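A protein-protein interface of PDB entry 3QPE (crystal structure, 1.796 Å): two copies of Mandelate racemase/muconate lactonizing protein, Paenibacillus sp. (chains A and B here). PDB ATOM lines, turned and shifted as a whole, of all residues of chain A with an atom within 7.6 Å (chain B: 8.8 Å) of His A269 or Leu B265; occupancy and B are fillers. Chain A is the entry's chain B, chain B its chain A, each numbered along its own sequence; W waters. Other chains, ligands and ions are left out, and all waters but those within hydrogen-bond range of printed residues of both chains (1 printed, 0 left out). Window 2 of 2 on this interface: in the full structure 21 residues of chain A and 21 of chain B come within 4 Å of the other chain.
NE2 of His A237 is in hydrogen-bond range of NE2 of His B237 (3.4 Å).
The side-chain carboxylate (OE1) of Glu A238 is in hydrogen-bond range of the backbone NH (N) of Ser A267 (2.8 Å).
The backbone NH (N) of His B237 lies within hydrogen-bond range of the side-chain amide oxygen (OD1) of Asn B210 (3.1 Å).
OE1 of Glu B238 is in hydrogen-bond range of N of Ser B267, 3.0 Å away.
A ring nitrogen (ND1) of His B237 lies close to the side-chain carboxylate of Glu B238 (3.3 Å).
OG of Ser A267 lies close to N of His A269 (3.4 Å).
OE2 of Glu A238 lies close to ND1 of His A237, at 3.4 Å.
Among the printed residues, merely in contact across the chains: Leu A265 with Ser B267 (3.5 Å), Ser A267 with Leu B265 (3.6 Å) and His A269 with Leu B265 (3.98 Å).
His A269 touches just one residue of chain B: Leu B265 (3.98 Å).
Leu B265 touches just these residues of chain A: Ser A267 (3.6 Å) and His A269 (3.98 Å).
Of the printed residues of chain B, His A237 touches His B237.
Of the printed residues of chain B, Leu A265 touches Ser B267.
Printed residues of chain A that touch a printed residue of chain B: His A237, Leu A265, Ser A267 and His A269.
Of the 17 printed residues of chain B, 3 touch a printed residue of chain A.
Hydrophobic or aromatic side chains of chain B within 4 Å of the printed part of chain A: His B237 and Leu B265.
His A237 touches its own counterpart, His B237.
Leu A265 touches Ser B267, and with the chains exchanged Ser A267 touches Leu B265.
Positions printed for both chains: 237, 238, 265, 266, 267, 268, 270 and 284.
Of the 4 pairs that touch across the chains among the printed residues, 3 have their exchanged pair printed and touching as well.
Water W1 bridges a ring nitrogen (NE2) of His A237 (2.8 Å) and the backbone carbonyl oxygen of Leu B265 (3.4 Å).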
ATOM      1  N   HIS A 237     -28.258   6.784  10.485  1.00  0.00           N
ATOM      2  CA  HIS A 237     -28.288   5.359  10.149  1.00  0.00           C
ATOM      3  C   HIS A 237     -29.733   4.890  10.096  1.00  0.00           C
ATOM      4  O   HIS A 237     -30.518   5.215  10.977  1.00  0.00           O
ATOM      5  CB  HIS A 237     -27.487   4.514  11.136  1.00  0.00           C
ATOM      6  CG  HIS A 237     -27.484   3.051  10.806  1.00  0.00           C
ATOM      7  ND1 HIS A 237     -26.893   2.547   9.667  1.00  0.00           N
ATOM      8  CD2 HIS A 237     -28.001   1.987  11.464  1.00  0.00           C
ATOM      9  CE1 HIS A 237     -27.045   1.235   9.639  1.00  0.00           C
ATOM     10  NE2 HIS A 237     -27.710   0.868  10.719  1.00  0.00           N
ATOM     11  N   GLU A 238     -30.074   4.117   9.070  1.00  0.00           N
ATOM     12  CA  GLU A 238     -31.460   3.706   8.853  1.00  0.00           C
ATOM     13  C   GLU A 238     -32.090   3.107  10.101  1.00  0.00           C
ATOM     14  O   GLU A 238     -31.505   2.253  10.762  1.00  0.00           O
ATOM     15  CB  GLU A 238     -31.585   2.745   7.666  1.00  0.00           C
ATOM     16  CG  GLU A 238     -30.678   1.536   7.737  1.00  0.00           C
ATOM     17  CD  GLU A 238     -29.397   1.754   6.974  1.00  0.00           C
ATOM     18  OE1 GLU A 238     -28.876   0.783   6.376  1.00  0.00           O
ATOM     19  OE2 GLU A 238     -28.919   2.906   6.971  1.00  0.00           O
ATOM     20  N   GLU A 240     -36.235   2.188  11.345  1.00  0.00           N
ATOM     21  CA  GLU A 240     -37.613   2.179  10.881  1.00  0.00           C
ATOM     22  C   GLU A 240     -38.459   3.175  11.651  1.00  0.00           C
ATOM     23  O   GLU A 240     -39.259   3.884  11.066  1.00  0.00           O
ATOM     24  CB  GLU A 240     -38.243   0.778  10.964  1.00  0.00           C
ATOM     25  CG  GLU A 240     -39.684   0.735  10.454  1.00  0.00           C
ATOM     26  CD  GLU A 240     -40.294  -0.667  10.446  1.00  0.00           C
ATOM     27  OE1 GLU A 240     -39.730  -1.598  11.063  1.00  0.00           O
ATOM     28  OE2 GLU A 240     -41.348  -0.835   9.805  1.00  0.00           O
ATOM     29  N   LEU A 265     -22.475  -0.719   5.197  1.00  0.00           N
ATOM     30  CA  LEU A 265     -22.995  -1.809   6.014  1.00  0.00           C
ATOM     31  C   LEU A 265     -24.430  -1.495   6.396  1.00  0.00           C
ATOM     32  O   LEU A 265     -24.681  -1.029   7.509  1.00  0.00           O
ATOM     33  CB  LEU A 265     -22.163  -1.955   7.290  1.00  0.00           C
ATOM     34  CG  LEU A 265     -20.668  -2.224   7.102  1.00  0.00           C
ATOM     35  CD1 LEU A 265     -19.893  -1.948   8.392  1.00  0.00           C
ATOM     36  CD2 LEU A 265     -20.447  -3.650   6.612  1.00  0.00           C
ATOM     37  N   ALA A 266     -25.354  -1.739   5.468  1.00  0.00           N
ATOM     38  CA  ALA A 266     -26.772  -1.400   5.639  1.00  0.00           C
ATOM     39  C   ALA A 266     -27.484  -2.322   6.624  1.00  0.00           C
ATOM     40  O   ALA A 266     -27.064  -3.453   6.841  1.00  0.00           O
ATOM     41  CB  ALA A 266     -27.485  -1.425   4.290  1.00  0.00           C
ATOM     42  N   SER A 267     -28.567  -1.839   7.226  1.00  0.00           N
ATOM     43  CA  SER A 267     -29.381  -2.703   8.084  1.00  0.00           C
ATOM     44  C   SER A 267     -29.890  -3.925   7.318  1.00  0.00           C
ATOM     45  O   SER A 267     -30.367  -3.795   6.195  1.00  0.00           O
ATOM     46  CB  SER A 267     -30.590  -1.952   8.620  1.00  0.00           C
ATOM     47  OG  SER A 267     -31.355  -2.808   9.450  1.00  0.00           O
ATOM     48  N   PRO A 268     -29.809  -5.115   7.934  1.00  0.00           N
ATOM     49  CA  PRO A 268     -30.264  -6.355   7.291  1.00  0.00           C
ATOM     50  C   PRO A 268     -31.755  -6.313   6.964  1.00  0.00           C
ATOM     51  O   PRO A 268     -32.251  -7.124   6.184  1.00  0.00           O
ATOM     52  CB  PRO A 268     -30.006  -7.419   8.360  1.00  0.00           C
ATOM     53  CG  PRO A 268     -28.929  -6.852   9.218  1.00  0.00           C
ATOM     54  CD  PRO A 268     -29.151  -5.367   9.228  1.00  0.00           C
ATOM     55  N   HIS A 269     -32.468  -5.371   7.561  1.00  0.00           N
ATOM     56  CA  HIS A 269     -33.901  -5.289   7.364  1.00  0.00           C
ATOM     57  C   HIS A 269     -34.282  -4.071   6.526  1.00  0.00           C
ATOM     58  O   HIS A 269     -35.460  -3.733   6.422  1.00  0.00           O
ATOM     59  CB  HIS A 269     -34.608  -5.244   8.719  1.00  0.00           C
ATOM     60  CG  HIS A 269     -34.285  -6.405   9.608  1.00  0.00           C
ATOM     61  ND1 HIS A 269     -34.667  -6.459  10.930  1.00  0.00           N
ATOM     62  CD2 HIS A 269     -33.624  -7.559   9.362  1.00  0.00           C
ATOM     63  CE1 HIS A 269     -34.251  -7.594  11.462  1.00  0.00           C
ATOM     64  NE2 HIS A 269     -33.614  -8.280  10.532  1.00  0.00           N
ATOM     65  N   LEU A 270     -33.299  -3.409   5.921  1.00  0.00           N
ATOM     66  CA  LEU A 270     -33.609  -2.189   5.178  1.00  0.00           C
ATOM     67  C   LEU A 270     -34.741  -2.373   4.158  1.00  0.00           C
ATOM     68  O   LEU A 270     -35.662  -1.549   4.082  1.00  0.00           O
ATOM     69  CB  LEU A 270     -32.365  -1.595   4.503  1.00  0.00           C
ATOM     70  CG  LEU A 270     -32.674  -0.382   3.615  1.00  0.00           C
ATOM     71  CD1 LEU A 270     -33.434   0.722   4.380  1.00  0.00           C
ATOM     72  CD2 LEU A 270     -31.425   0.195   2.960  1.00  0.00           C
ATOM     73  N   ILE A 271     -34.688  -3.444   3.373  1.00  0.00           N
ATOM     74  CA  ILE A 271     -35.685  -3.629   2.315  1.00  0.00           C
ATOM     75  C   ILE A 271     -37.104  -3.819   2.862  1.00  0.00           C
ATOM     76  O   ILE A 271     -38.065  -3.228   2.351  1.00  0.00           O
ATOM     77  CB  ILE A 271     -35.306  -4.773   1.352  1.00  0.00           C
ATOM     78  CG1 ILE A 271     -34.112  -4.354   0.487  1.00  0.00           C
ATOM     79  CG2 ILE A 271     -36.484  -5.105   0.455  1.00  0.00           C
ATOM     80  CD1 ILE A 271     -33.260  -5.502   0.018  1.00  0.00           C
ATOM     81  N   GLU A 272     -37.229  -4.629   3.906  1.00  0.00           N
ATOM     82  CA  GLU A 272     -38.503  -4.812   4.597  1.00  0.00           C
ATOM     83  C   GLU A 272     -39.095  -3.466   5.018  1.00  0.00           C
ATOM     84  O   GLU A 272     -40.254  -3.163   4.741  1.00  0.00           O
ATOM     85  CB  GLU A 272     -38.281  -5.686   5.820  1.00  0.00           C
ATOM     86  CG  GLU A 272     -39.519  -5.994   6.613  1.00  0.00           C
ATOM     87  CD  GLU A 272     -39.211  -6.903   7.784  1.00  0.00           C
ATOM     88  OE1 GLU A 272     -38.025  -7.269   7.950  1.00  0.00           O
ATOM     89  OE2 GLU A 272     -40.150  -7.253   8.534  1.00  0.00           O
ATOM     90  N   TRP A 273     -38.280  -2.659   5.686  1.00  0.00           N
ATOM     91  CA  TRP A 273     -38.685  -1.330   6.099  1.00  0.00           C
ATOM     92  C   TRP A 273     -39.196  -0.529   4.904  1.00  0.00           C
ATOM     93  O   TRP A 273     -40.174   0.200   5.014  1.00  0.00           O
ATOM     94  CB  TRP A 273     -37.503  -0.591   6.732  1.00  0.00           C
ATOM     95  CG  TRP A 273     -36.960  -1.219   7.982  1.00  0.00           C
ATOM     96  CD1 TRP A 273     -37.536  -2.209   8.727  1.00  0.00           C
ATOM     97  CD2 TRP A 273     -35.725  -0.891   8.636  1.00  0.00           C
ATOM     98  NE1 TRP A 273     -36.737  -2.518   9.802  1.00  0.00           N
ATOM     99  CE2 TRP A 273     -35.620  -1.723   9.770  1.00  0.00           C
ATOM    100  CE3 TRP A 273     -34.697   0.031   8.372  1.00  0.00           C
ATOM    101  CZ2 TRP A 273     -34.533  -1.665  10.639  1.00  0.00           C
ATOM    102  CZ3 TRP A 273     -33.616   0.082   9.231  1.00  0.00           C
ATOM    103  CH2 TRP A 273     -33.543  -0.760  10.354  1.00  0.00           C
ATOM    104  N   ALA A 274     -38.514  -0.657   3.770  1.00  0.00           N
ATOM    105  CA  ALA A 274     -38.896   0.045   2.548  1.00  0.00           C
ATOM    106  C   ALA A 274     -40.252  -0.454   2.022  1.00  0.00           C
ATOM    107  O   ALA A 274     -41.088   0.341   1.565  1.00  0.00           O
ATOM    108  CB  ALA A 274     -37.825  -0.134   1.489  1.00  0.00           C
ATOM    109  N   THR A 275     -40.462  -1.764   2.094  1.00  0.00           N
ATOM    110  CA  THR A 275     -41.718  -2.357   1.634  1.00  0.00           C
ATOM    111  C   THR A 275     -42.878  -1.860   2.482  1.00  0.00           C
ATOM    112  O   THR A 275     -44.032  -1.929   2.064  1.00  0.00           O
ATOM    113  CB  THR A 275     -41.701  -3.917   1.645  1.00  0.00           C
ATOM    114  OG1 THR A 275     -41.655  -4.411   2.992  1.00  0.00           O
ATOM    115  CG2 THR A 275     -40.517  -4.458   0.859  1.00  0.00           C
ATOM    116  N   ARG A 276     -42.568  -1.357   3.673  1.00  0.00           N
ATOM    117  CA  ARG A 276     -43.594  -0.815   4.553  1.00  0.00           C
ATOM    118  C   ARG A 276     -43.665   0.705   4.458  1.00  0.00           C
ATOM    119  O   ARG A 276     -44.287   1.357   5.293  1.00  0.00           O
ATOM    120  CB  ARG A 276     -43.378  -1.279   5.998  1.00  0.00           C
ATOM    121  CG  ARG A 276     -43.591  -2.768   6.183  1.00  0.00           C
ATOM    122  CD  ARG A 276     -43.774  -3.133   7.644  1.00  0.00           C
ATOM    123  NE  ARG A 276     -42.516  -3.019   8.370  1.00  0.00           N
ATOM    124  CZ  ARG A 276     -41.737  -4.045   8.691  1.00  0.00           C
ATOM    125  NH1 ARG A 276     -42.088  -5.280   8.363  1.00  0.00           N
ATOM    126  NH2 ARG A 276     -40.606  -3.833   9.348  1.00  0.00           N
ATOM    127  N   TYR A 284     -27.846   0.204  -2.616  1.00  0.00           N
ATOM    128  CA  TYR A 284     -26.769  -0.771  -2.583  1.00  0.00           C
ATOM    129  C   TYR A 284     -25.770  -0.470  -3.698  1.00  0.00           C
ATOM    130  O   TYR A 284     -26.165  -0.060  -4.783  1.00  0.00           O
ATOM    131  CB  TYR A 284     -27.341  -2.183  -2.703  1.00  0.00           C
ATOM    132  CG  TYR A 284     -28.342  -2.465  -1.614  1.00  0.00           C
ATOM    133  CD1 TYR A 284     -27.925  -2.843  -0.347  1.00  0.00           C
ATOM    134  CD2 TYR A 284     -29.697  -2.310  -1.835  1.00  0.00           C
ATOM    135  CE1 TYR A 284     -28.836  -3.079   0.663  1.00  0.00           C
ATOM    136  CE2 TYR A 284     -30.621  -2.543  -0.831  1.00  0.00           C
ATOM    137  CZ  TYR A 284     -30.184  -2.929   0.410  1.00  0.00           C
ATOM    138  OH  TYR A 284     -31.092  -3.155   1.410  1.00  0.00           O
ATOM    139  N   ARG B  35     -34.909   6.941  20.754  1.00  0.00           N
ATOM    140  CA  ARG B  35     -35.457   6.635  19.428  1.00  0.00           C
ATOM    141  C   ARG B  35     -36.943   6.285  19.373  1.00  0.00           C
ATOM    142  O   ARG B  35     -37.577   6.462  18.331  1.00  0.00           O
ATOM    143  CB  ARG B  35     -34.666   5.502  18.759  1.00  0.00           C
ATOM    144  CG  ARG B  35     -34.482   4.239  19.615  1.00  0.00           C
ATOM    145  CD  ARG B  35     -33.733   3.134  18.839  1.00  0.00           C
ATOM    146  NE  ARG B  35     -34.441   2.773  17.612  1.00  0.00           N
ATOM    147  CZ  ARG B  35     -35.375   1.830  17.538  1.00  0.00           C
ATOM    148  NH1 ARG B  35     -35.982   1.584  16.386  1.00  0.00           N
ATOM    149  NH2 ARG B  35     -35.708   1.132  18.617  1.00  0.00           N
ATOM    150  N   ASN B 210     -28.408   5.953  20.030  1.00  0.00           N
ATOM    151  CA  ASN B 210     -28.021   6.388  18.698  1.00  0.00           C
ATOM    152  C   ASN B 210     -28.573   7.749  18.321  1.00  0.00           C
ATOM    153  O   ASN B 210     -28.490   8.169  17.166  1.00  0.00           O
ATOM    154  CB  ASN B 210     -28.407   5.332  17.660  1.00  0.00           C
ATOM    155  CG  ASN B 210     -27.501   4.106  17.721  1.00  0.00           C
ATOM    156  OD1 ASN B 210     -26.381   4.185  18.204  1.00  0.00           O
ATOM    157  ND2 ASN B 210     -27.989   2.975  17.233  1.00  0.00           N
ATOM    158  N   GLU B 234     -23.798   3.581  22.792  1.00  0.00           N
ATOM    159  CA  GLU B 234     -24.546   3.915  21.583  1.00  0.00           C
ATOM    160  C   GLU B 234     -24.805   5.417  21.377  1.00  0.00           C
ATOM    161  O   GLU B 234     -25.940   5.831  21.164  1.00  0.00           O
ATOM    162  CB  GLU B 234     -25.868   3.144  21.527  1.00  0.00           C
ATOM    163  CG  GLU B 234     -25.696   1.624  21.450  1.00  0.00           C
ATOM    164  CD  GLU B 234     -26.830   0.942  20.676  1.00  0.00           C
ATOM    165  OE1 GLU B 234     -28.007   1.057  21.061  1.00  0.00           O
ATOM    166  OE2 GLU B 234     -26.557   0.278  19.670  1.00  0.00           O
ATOM    167  N   HIS B 237     -24.916   5.302  15.710  1.00  0.00           N
ATOM    168  CA  HIS B 237     -24.689   3.955  15.212  1.00  0.00           C
ATOM    169  C   HIS B 237     -23.195   3.750  14.965  1.00  0.00           C
ATOM    170  O   HIS B 237     -22.547   4.596  14.355  1.00  0.00           O
ATOM    171  CB  HIS B 237     -25.472   3.671  13.936  1.00  0.00           C
ATOM    172  CG  HIS B 237     -25.271   2.279  13.436  1.00  0.00           C
ATOM    173  ND1 HIS B 237     -25.600   1.175  14.189  1.00  0.00           N
ATOM    174  CD2 HIS B 237     -24.717   1.807  12.294  1.00  0.00           C
ATOM    175  CE1 HIS B 237     -25.287   0.078  13.519  1.00  0.00           C
ATOM    176  NE2 HIS B 237     -24.745   0.436  12.366  1.00  0.00           N
ATOM    177  N   GLU B 238     -22.663   2.626  15.439  1.00  0.00           N
ATOM    178  CA  GLU B 238     -21.226   2.378  15.405  1.00  0.00           C
ATOM    179  C   GLU B 238     -20.596   2.610  14.024  1.00  0.00           C
ATOM    180  O   GLU B 238     -21.117   2.176  12.998  1.00  0.00           O
ATOM    181  CB  GLU B 238     -20.878   0.979  15.924  1.00  0.00           C
ATOM    182  CG  GLU B 238     -21.618  -0.150  15.237  1.00  0.00           C
ATOM    183  CD  GLU B 238     -22.852  -0.555  16.007  1.00  0.00           C
ATOM    184  OE1 GLU B 238     -23.216  -1.751  16.004  1.00  0.00           O
ATOM    185  OE2 GLU B 238     -23.451   0.344  16.613  1.00  0.00           O
ATOM    186  N   ASP B 261     -20.963  -0.505  23.080  1.00  0.00           N
ATOM    187  CA  ASP B 261     -21.827  -0.661  21.918  1.00  0.00           C
ATOM    188  C   ASP B 261     -22.077  -2.153  21.641  1.00  0.00           C
ATOM    189  O   ASP B 261     -21.470  -2.986  22.276  1.00  0.00           O
ATOM    190  CB  ASP B 261     -21.216   0.045  20.709  1.00  0.00           C
ATOM    191  CG  ASP B 261     -22.269   0.666  19.818  1.00  0.00           C
ATOM    192  OD1 ASP B 261     -23.348   0.056  19.697  1.00  0.00           O
ATOM    193  OD2 ASP B 261     -22.038   1.760  19.263  1.00  0.00           O
ATOM    194  N   GLY B 262     -23.002  -2.473  20.738  1.00  0.00           N
ATOM    195  CA  GLY B 262     -23.173  -3.848  20.289  1.00  0.00           C
ATOM    196  C   GLY B 262     -24.572  -4.446  20.365  1.00  0.00           C
ATOM    197  O   GLY B 262     -24.803  -5.525  19.835  1.00  0.00           O
ATOM    198  N   GLU B 263     -25.514  -3.775  21.024  1.00  0.00           N
ATOM    199  CA  GLU B 263     -26.881  -4.323  21.089  1.00  0.00           C
ATOM    200  C   GLU B 263     -27.601  -4.252  19.734  1.00  0.00           C
ATOM    201  O   GLU B 263     -27.205  -3.491  18.839  1.00  0.00           O
ATOM    202  CB  GLU B 263     -27.715  -3.617  22.176  1.00  0.00           C
ATOM    203  CG  GLU B 263     -28.228  -2.257  21.763  1.00  0.00           C
ATOM    204  CD  GLU B 263     -28.911  -1.531  22.911  1.00  0.00           C
ATOM    205  OE1 GLU B 263     -30.090  -1.138  22.758  1.00  0.00           O
ATOM    206  OE2 GLU B 263     -28.259  -1.375  23.966  1.00  0.00           O
ATOM    207  N   GLY B 264     -28.641  -5.073  19.578  1.00  0.00           N
ATOM    208  CA  GLY B 264     -29.466  -5.059  18.380  1.00  0.00           C
ATOM    209  C   GLY B 264     -28.739  -5.479  17.113  1.00  0.00           C
ATOM    210  O   GLY B 264     -27.930  -6.404  17.129  1.00  0.00           O
ATOM    211  N   LEU B 265     -29.023  -4.796  16.006  1.00  0.00           N
ATOM    212  CA  LEU B 265     -28.413  -5.153  14.730  1.00  0.00           C
ATOM    213  C   LEU B 265     -27.063  -4.461  14.628  1.00  0.00           C
ATOM    214  O   LEU B 265     -26.968  -3.335  14.113  1.00  0.00           O
ATOM    215  CB  LEU B 265     -29.308  -4.717  13.570  1.00  0.00           C
ATOM    216  CG  LEU B 265     -30.723  -5.301  13.541  1.00  0.00           C
ATOM    217  CD1 LEU B 265     -31.593  -4.533  12.564  1.00  0.00           C
ATOM    218  CD2 LEU B 265     -30.666  -6.785  13.193  1.00  0.00           C
ATOM    219  N   ALA B 266     -26.027  -5.118  15.147  1.00  0.00           N
ATOM    220  CA  ALA B 266     -24.686  -4.516  15.209  1.00  0.00           C
ATOM    221  C   ALA B 266     -23.956  -4.573  13.873  1.00  0.00           C
ATOM    222  O   ALA B 266     -24.210  -5.452  13.061  1.00  0.00           O
ATOM    223  CB  ALA B 266     -23.855  -5.194  16.285  1.00  0.00           C
ATOM    224  N   SER B 267     -23.043  -3.634  13.648  1.00  0.00           N
ATOM    225  CA  SER B 267     -22.138  -3.756  12.524  1.00  0.00           C
ATOM    226  C   SER B 267     -21.415  -5.091  12.620  1.00  0.00           C
ATOM    227  O   SER B 267     -20.954  -5.471  13.686  1.00  0.00           O
ATOM    228  CB  SER B 267     -21.114  -2.627  12.539  1.00  0.00           C
ATOM    229  OG  SER B 267     -19.998  -2.978  11.740  1.00  0.00           O
ATOM    230  N   PRO B 268     -21.306  -5.811  11.497  1.00  0.00           N
ATOM    231  CA  PRO B 268     -20.577  -7.081  11.473  1.00  0.00           C
ATOM    232  C   PRO B 268     -19.101  -6.908  11.811  1.00  0.00           C
ATOM    233  O   PRO B 268     -18.431  -7.900  12.092  1.00  0.00           O
ATOM    234  CB  PRO B 268     -20.708  -7.536  10.017  1.00  0.00           C
ATOM    235  CG  PRO B 268     -21.840  -6.742   9.452  1.00  0.00           C
ATOM    236  CD  PRO B 268     -21.802  -5.435  10.165  1.00  0.00           C
ATOM    237  N   LEU B 270     -17.910  -4.742  14.234  1.00  0.00           N
ATOM    238  CA  LEU B 270     -17.774  -4.116  15.548  1.00  0.00           C
ATOM    239  C   LEU B 270     -16.633  -4.705  16.381  1.00  0.00           C
ATOM    240  O   LEU B 270     -15.865  -3.975  16.997  1.00  0.00           O
ATOM    241  CB  LEU B 270     -19.091  -4.242  16.330  1.00  0.00           C
ATOM    242  CG  LEU B 270     -19.040  -3.574  17.704  1.00  0.00           C
ATOM    243  CD1 LEU B 270     -18.813  -2.070  17.554  1.00  0.00           C
ATOM    244  CD2 LEU B 270     -20.349  -3.836  18.465  1.00  0.00           C
ATOM    245  N   TYR B 284     -23.584  -7.404  23.193  1.00  0.00           N
ATOM    246  CA  TYR B 284     -24.514  -8.373  22.615  1.00  0.00           C
ATOM    247  C   TYR B 284     -25.467  -8.900  23.684  1.00  0.00           C
ATOM    248  O   TYR B 284     -25.078  -9.113  24.835  1.00  0.00           O
ATOM    249  CB  TYR B 284     -23.762  -9.525  21.941  1.00  0.00           C
ATOM    250  CG  TYR B 284     -22.814  -9.010  20.877  1.00  0.00           C
ATOM    251  CD1 TYR B 284     -23.274  -8.706  19.601  1.00  0.00           C
ATOM    252  CD2 TYR B 284     -21.478  -8.777  21.165  1.00  0.00           C
ATOM    253  CE1 TYR B 284     -22.427  -8.206  18.632  1.00  0.00           C
ATOM    254  CE2 TYR B 284     -20.615  -8.270  20.193  1.00  0.00           C
ATOM    255  CZ  TYR B 284     -21.097  -7.992  18.931  1.00  0.00           C
ATOM    256  OH  TYR B 284     -20.250  -7.489  17.963  1.00  0.00           O
ATOM    257  N   ASP B 285     -26.710  -9.124  23.283  1.00  0.00           N
ATOM    258  CA  ASP B 285     -27.785  -9.484  24.209  1.00  0.00           C
ATOM    259  C   ASP B 285     -27.584 -10.863  24.874  1.00  0.00           C
ATOM    260  O   ASP B 285     -26.979 -11.769  24.294  1.00  0.00           O
ATOM    261  CB  ASP B 285     -29.114  -9.397  23.450  1.00  0.00           C
ATOM    262  CG  ASP B 285     -30.314  -9.748  24.310  1.00  0.00           C
ATOM    263  OD1 ASP B 285     -30.869  -8.834  24.971  1.00  0.00           O
ATOM    264  OD2 ASP B 285     -30.723 -10.916  24.280  1.00  0.00           O
ATOM    265  N   TRP B 288     -30.134 -13.442  22.834  1.00  0.00           N
ATOM    266  CA  TRP B 288     -29.785 -13.582  21.434  1.00  0.00           C
ATOM    267  C   TRP B 288     -28.607 -12.648  21.160  1.00  0.00           C
ATOM    268  O   TRP B 288     -28.774 -11.424  21.156  1.00  0.00           O
ATOM    269  CB  TRP B 288     -31.003 -13.243  20.559  1.00  0.00           C
ATOM    270  CG  TRP B 288     -30.694 -13.262  19.106  1.00  0.00           C
ATOM    271  CD1 TRP B 288     -30.824 -14.315  18.253  1.00  0.00           C
ATOM    272  CD2 TRP B 288     -30.161 -12.179  18.331  1.00  0.00           C
ATOM    273  NE1 TRP B 288     -30.421 -13.959  16.990  1.00  0.00           N
ATOM    274  CE2 TRP B 288     -30.003 -12.652  17.010  1.00  0.00           C
ATOM    275  CE3 TRP B 288     -29.809 -10.852  18.622  1.00  0.00           C
ATOM    276  CZ2 TRP B 288     -29.508 -11.845  15.980  1.00  0.00           C
ATOM    277  CZ3 TRP B 288     -29.314 -10.055  17.599  1.00  0.00           C
ATOM    278  CH2 TRP B 288     -29.172 -10.555  16.294  1.00  0.00           C
HETATM  279  O   HOH W   1     -28.253  -1.775  11.403  1.00  0.00           O
